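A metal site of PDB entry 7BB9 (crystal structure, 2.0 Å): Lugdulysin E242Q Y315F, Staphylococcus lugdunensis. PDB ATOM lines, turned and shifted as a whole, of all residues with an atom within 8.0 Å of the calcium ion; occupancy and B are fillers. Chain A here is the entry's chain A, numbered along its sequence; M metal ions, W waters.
OG of Ser 141 lies within hydrogen-bond range of OE2 of Glu 186, 2.7 Å away. The backbone NH (N) of Val 143 lies within hydrogen-bond range of the side-chain carboxylate (OE2) of Glu 186 (2.7 Å). N of Asn 150 sits at hydrogen-bond distance from O of Glu 186 (2.7 Å). N of Gly 147 sits at hydrogen-bond distance from OD2 of Asp 142, at 2.9 Å. The side-chain carboxylate (OD1) of Asp 142 lies close to the backbone NH (N) of Asn 145 (3.2 Å).
Five residues have an atom within 4 Å of the calcium ion: Asp 142, Asp 144, Asn 146, Lys 148 and Glu 186.
The calcium ion is bound by the side-chain carboxylate (OE1) of Glu 186 (2.3 Å), the side-chain carboxylate (OD1) of Asp 142 (2.4 Å), the side-chain carboxylate (OD1) of Asp 144 (2.4 Å), the backbone carbonyl oxygen (O) of Lys 148 (2.4 Å), the side-chain amide oxygen (OD1) of Asn 146 (2.4 Å), water W2 (2.5 Å) and water W1 (2.5 Å). The calcium ion has seven donor atoms within binding distance.
Water W1 bridges OD2 of Asp 144 (2.6 Å) and N of Glu 186 (3.4 Å).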
ATOM      1  N   LYS A 103      26.125 -14.306 -19.896  1.00  0.00           N
ATOM      2  CA  LYS A 103      27.091 -14.795 -20.874  1.00  0.00           C
ATOM      3  C   LYS A 103      27.590 -16.197 -20.534  1.00  0.00           C
ATOM      4  O   LYS A 103      27.854 -17.000 -21.423  1.00  0.00           O
ATOM      5  CB  LYS A 103      28.276 -13.851 -20.985  1.00  0.00           C
ATOM      6  CG  LYS A 103      29.280 -14.258 -22.053  1.00  0.00           C
ATOM      7  CD  LYS A 103      28.903 -13.632 -23.386  1.00  0.00           C
ATOM      8  CE  LYS A 103      30.102 -13.354 -24.238  1.00  0.00           C
ATOM      9  NZ  LYS A 103      30.355 -11.892 -24.301  1.00  0.00           N
ATOM     10  N   GLN A 105      27.373 -20.016 -18.975  1.00  0.00           N
ATOM     11  CA  GLN A 105      26.625 -21.153 -18.449  1.00  0.00           C
ATOM     12  C   GLN A 105      27.597 -22.054 -17.692  1.00  0.00           C
ATOM     13  O   GLN A 105      28.531 -22.606 -18.287  1.00  0.00           O
ATOM     14  CB  GLN A 105      25.916 -21.886 -19.585  1.00  0.00           C
ATOM     15  CG  GLN A 105      24.816 -21.067 -20.221  1.00  0.00           C
ATOM     16  CD  GLN A 105      23.994 -21.871 -21.212  1.00  0.00           C
ATOM     17  OE1 GLN A 105      24.545 -22.595 -22.050  1.00  0.00           O
ATOM     18  NE2 GLN A 105      22.671 -21.758 -21.122  1.00  0.00           N
ATOM     19  N   PRO A 140      34.610 -13.909 -28.063  1.00  0.00           N
ATOM     20  CA  PRO A 140      34.480 -15.332 -28.385  1.00  0.00           C
ATOM     21  C   PRO A 140      33.722 -15.554 -29.690  1.00  0.00           C
ATOM     22  O   PRO A 140      33.076 -14.653 -30.234  1.00  0.00           O
ATOM     23  CB  PRO A 140      33.687 -15.887 -27.201  1.00  0.00           C
ATOM     24  CG  PRO A 140      32.855 -14.742 -26.743  1.00  0.00           C
ATOM     25  CD  PRO A 140      33.686 -13.501 -26.986  1.00  0.00           C
ATOM     26  N   SER A 141      33.809 -16.787 -30.197  1.00  0.00           N
ATOM     27  CA  SER A 141      32.923 -17.250 -31.261  1.00  0.00           C
ATOM     28  C   SER A 141      31.546 -17.586 -30.695  1.00  0.00           C
ATOM     29  O   SER A 141      31.292 -17.475 -29.496  1.00  0.00           O
ATOM     30  CB  SER A 141      33.543 -18.471 -31.959  1.00  0.00           C
ATOM     31  OG  SER A 141      33.861 -19.473 -31.018  1.00  0.00           O
ATOM     32  N   ASP A 142      30.618 -17.999 -31.568  1.00  0.00           N
ATOM     33  CA  ASP A 142      29.315 -18.509 -31.134  1.00  0.00           C
ATOM     34  C   ASP A 142      28.877 -19.589 -32.105  1.00  0.00           C
ATOM     35  O   ASP A 142      27.872 -19.490 -32.807  1.00  0.00           O
ATOM     36  CB  ASP A 142      28.271 -17.384 -31.027  1.00  0.00           C
ATOM     37  CG  ASP A 142      27.018 -17.809 -30.264  1.00  0.00           C
ATOM     38  OD1 ASP A 142      27.022 -18.862 -29.575  1.00  0.00           O
ATOM     39  OD2 ASP A 142      26.018 -17.082 -30.352  1.00  0.00           O
ATOM     40  N   VAL A 143      29.644 -20.678 -32.140  1.00  0.00           N
ATOM     41  CA  VAL A 143      29.400 -21.749 -33.103  1.00  0.00           C
ATOM     42  C   VAL A 143      28.074 -22.446 -32.859  1.00  0.00           C
ATOM     43  O   VAL A 143      27.539 -23.088 -33.772  1.00  0.00           O
ATOM     44  CB  VAL A 143      30.570 -22.751 -33.090  1.00  0.00           C
ATOM     45  CG1 VAL A 143      31.838 -22.063 -33.552  1.00  0.00           C
ATOM     46  CG2 VAL A 143      30.767 -23.313 -31.697  1.00  0.00           C
ATOM     47  N   ASP A 144      27.505 -22.332 -31.671  1.00  0.00           N
ATOM     48  CA  ASP A 144      26.202 -22.922 -31.418  1.00  0.00           C
ATOM     49  C   ASP A 144      25.092 -21.876 -31.385  1.00  0.00           C
ATOM     50  O   ASP A 144      23.958 -22.208 -31.032  1.00  0.00           O
ATOM     51  CB  ASP A 144      26.227 -23.725 -30.118  1.00  0.00           C
ATOM     52  CG  ASP A 144      26.785 -22.952 -28.961  1.00  0.00           C
ATOM     53  OD1 ASP A 144      27.035 -21.732 -29.139  1.00  0.00           O
ATOM     54  OD2 ASP A 144      26.967 -23.549 -27.883  1.00  0.00           O
ATOM     55  N   ASN A 145      25.400 -20.620 -31.745  1.00  0.00           N
ATOM     56  CA  ASN A 145      24.400 -19.563 -31.836  1.00  0.00           C
ATOM     57  C   ASN A 145      23.492 -19.536 -30.608  1.00  0.00           C
ATOM     58  O   ASN A 145      22.267 -19.551 -30.706  1.00  0.00           O
ATOM     59  CB  ASN A 145      23.577 -19.718 -33.124  1.00  0.00           C
ATOM     60  CG  ASN A 145      22.756 -18.474 -33.458  1.00  0.00           C
ATOM     61  OD1 ASN A 145      23.133 -17.356 -33.119  1.00  0.00           O
ATOM     62  ND2 ASN A 145      21.634 -18.670 -34.144  1.00  0.00           N
ATOM     63  N   ASN A 146      24.102 -19.532 -29.414  1.00  0.00           N
ATOM     64  CA  ASN A 146      23.320 -19.418 -28.189  1.00  0.00           C
ATOM     65  C   ASN A 146      23.698 -18.197 -27.358  1.00  0.00           C
ATOM     66  O   ASN A 146      23.220 -18.047 -26.242  1.00  0.00           O
ATOM     67  CB  ASN A 146      23.423 -20.703 -27.348  1.00  0.00           C
ATOM     68  CG  ASN A 146      24.746 -20.859 -26.611  1.00  0.00           C
ATOM     69  OD1 ASN A 146      25.736 -20.160 -26.887  1.00  0.00           O
ATOM     70  ND2 ASN A 146      24.773 -21.784 -25.655  1.00  0.00           N
ATOM     71  N   GLY A 147      24.570 -17.331 -27.878  1.00  0.00           N
ATOM     72  CA  GLY A 147      24.966 -16.136 -27.155  1.00  0.00           C
ATOM     73  C   GLY A 147      25.763 -16.341 -25.878  1.00  0.00           C
ATOM     74  O   GLY A 147      26.043 -15.355 -25.189  1.00  0.00           O
ATOM     75  N   LYS A 148      26.140 -17.564 -25.534  1.00  0.00           N
ATOM     76  CA  LYS A 148      26.773 -17.819 -24.233  1.00  0.00           C
ATOM     77  C   LYS A 148      27.997 -18.721 -24.405  1.00  0.00           C
ATOM     78  O   LYS A 148      28.267 -19.266 -25.476  1.00  0.00           O
ATOM     79  CB  LYS A 148      25.742 -18.427 -23.261  1.00  0.00           C
ATOM     80  CG  LYS A 148      24.452 -17.585 -23.102  1.00  0.00           C
ATOM     81  CD  LYS A 148      23.635 -18.020 -21.864  1.00  0.00           C
ATOM     82  CE  LYS A 148      22.232 -17.418 -21.830  1.00  0.00           C
ATOM     83  NZ  LYS A 148      21.524 -17.756 -20.548  1.00  0.00           N
ATOM     84  N   VAL A 149      28.781 -18.870 -23.320  1.00  0.00           N
ATOM     85  CA  VAL A 149      29.904 -19.804 -23.316  1.00  0.00           C
ATOM     86  C   VAL A 149      29.774 -20.729 -22.116  1.00  0.00           C
ATOM     87  O   VAL A 149      29.301 -20.336 -21.048  1.00  0.00           O
ATOM     88  CB  VAL A 149      31.299 -19.108 -23.349  1.00  0.00           C
ATOM     89  CG1 VAL A 149      31.310 -17.928 -24.353  1.00  0.00           C
ATOM     90  CG2 VAL A 149      31.771 -18.677 -21.969  1.00  0.00           C
ATOM     91  N   ASN A 150      30.199 -21.981 -22.304  1.00  0.00           N
ATOM     92  CA  ASN A 150      30.103 -22.986 -21.260  1.00  0.00           C
ATOM     93  C   ASN A 150      31.364 -22.979 -20.405  1.00  0.00           C
ATOM     94  O   ASN A 150      32.482 -22.896 -20.919  1.00  0.00           O
ATOM     95  CB  ASN A 150      29.902 -24.392 -21.864  1.00  0.00           C
ATOM     96  CG  ASN A 150      28.638 -24.512 -22.664  1.00  0.00           C
ATOM     97  OD1 ASN A 150      27.576 -24.068 -22.237  1.00  0.00           O
ATOM     98  ND2 ASN A 150      28.758 -25.124 -23.845  1.00  0.00           N
ATOM     99  N   LEU A 176      35.234 -26.069 -31.360  1.00  0.00           N
ATOM    100  CA  LEU A 176      34.681 -25.108 -32.307  1.00  0.00           C
ATOM    101  C   LEU A 176      34.475 -25.677 -33.698  1.00  0.00           C
ATOM    102  O   LEU A 176      34.027 -24.948 -34.589  1.00  0.00           O
ATOM    103  CB  LEU A 176      35.587 -23.864 -32.391  1.00  0.00           C
ATOM    104  CG  LEU A 176      35.985 -23.271 -31.040  1.00  0.00           C
ATOM    105  CD1 LEU A 176      36.861 -22.033 -31.221  1.00  0.00           C
ATOM    106  CD2 LEU A 176      34.752 -22.959 -30.171  1.00  0.00           C
ATOM    107  N   HIS A 184      31.069 -29.042 -29.630  1.00  0.00           N
ATOM    108  CA  HIS A 184      30.271 -28.197 -30.527  1.00  0.00           C
ATOM    109  C   HIS A 184      29.826 -26.911 -29.841  1.00  0.00           C
ATOM    110  O   HIS A 184      28.660 -26.521 -29.890  1.00  0.00           O
ATOM    111  CB  HIS A 184      29.028 -28.957 -31.044  1.00  0.00           C
ATOM    112  CG  HIS A 184      29.318 -29.889 -32.169  1.00  0.00           C
ATOM    113  ND1 HIS A 184      28.329 -30.433 -32.961  1.00  0.00           N
ATOM    114  CD2 HIS A 184      30.483 -30.393 -32.632  1.00  0.00           C
ATOM    115  CE1 HIS A 184      28.872 -31.225 -33.865  1.00  0.00           C
ATOM    116  NE2 HIS A 184      30.187 -31.221 -33.687  1.00  0.00           N
ATOM    117  N   SER A 185      30.769 -26.231 -29.171  1.00  0.00           N
ATOM    118  CA  SER A 185      30.373 -25.018 -28.461  1.00  0.00           C
ATOM    119  C   SER A 185      31.601 -24.282 -27.967  1.00  0.00           C
ATOM    120  O   SER A 185      32.716 -24.799 -27.976  1.00  0.00           O
ATOM    121  CB  SER A 185      29.427 -25.328 -27.288  1.00  0.00           C
ATOM    122  OG  SER A 185      30.054 -26.160 -26.340  1.00  0.00           O
ATOM    123  N   GLU A 186      31.375 -23.038 -27.569  1.00  0.00           N
ATOM    124  CA  GLU A 186      32.317 -22.302 -26.737  1.00  0.00           C
ATOM    125  C   GLU A 186      32.298 -22.911 -25.342  1.00  0.00           C
ATOM    126  O   GLU A 186      31.292 -22.830 -24.632  1.00  0.00           O
ATOM    127  CB  GLU A 186      31.947 -20.826 -26.683  1.00  0.00           C
ATOM    128  CG  GLU A 186      32.174 -20.088 -27.993  1.00  0.00           C
ATOM    129  CD  GLU A 186      31.157 -20.452 -29.062  1.00  0.00           C
ATOM    130  OE1 GLU A 186      29.957 -20.586 -28.732  1.00  0.00           O
ATOM    131  OE2 GLU A 186      31.561 -20.597 -30.241  1.00  0.00           O
ATOM    132  N   ILE A 187      33.400 -23.532 -24.942  1.00  0.00           N
ATOM    133  CA  ILE A 187      33.490 -24.113 -23.608  1.00  0.00           C
ATOM    134  C   ILE A 187      34.934 -24.051 -23.174  1.00  0.00           C
ATOM    135  O   ILE A 187      35.842 -24.212 -23.992  1.00  0.00           O
ATOM    136  CB  ILE A 187      32.945 -25.559 -23.594  1.00  0.00           C
ATOM    137  CG1 ILE A 187      33.209 -26.243 -22.249  1.00  0.00           C
ATOM    138  CG2 ILE A 187      33.564 -26.354 -24.730  1.00  0.00           C
ATOM    139  CD1 ILE A 187      32.437 -27.580 -22.073  1.00  0.00           C
ATOM    140  N   MET A 219      40.224 -18.724 -25.407  1.00  0.00           N
ATOM    141  CA  MET A 219      39.014 -18.902 -26.217  1.00  0.00           C
ATOM    142  C   MET A 219      38.859 -17.789 -27.250  1.00  0.00           C
ATOM    143  O   MET A 219      38.621 -18.053 -28.433  1.00  0.00           O
ATOM    144  CB  MET A 219      37.767 -18.954 -25.333  1.00  0.00           C
ATOM    145  CG  MET A 219      36.428 -19.001 -26.090  1.00  0.00           C
ATOM    146  SD  MET A 219      34.985 -19.184 -24.992  1.00  0.00           S
ATOM    147  CE  MET A 219      35.239 -20.882 -24.466  1.00  0.00           C
HETATM  148 CA    CA M   1      28.002 -20.033 -27.744  1.00  0.00          CA
HETATM  149  O   HOH W   1      28.440 -22.043 -26.286  1.00  0.00           O
HETATM  150  O   HOH W   2      29.254 -17.860 -27.701  1.00  0.00           O
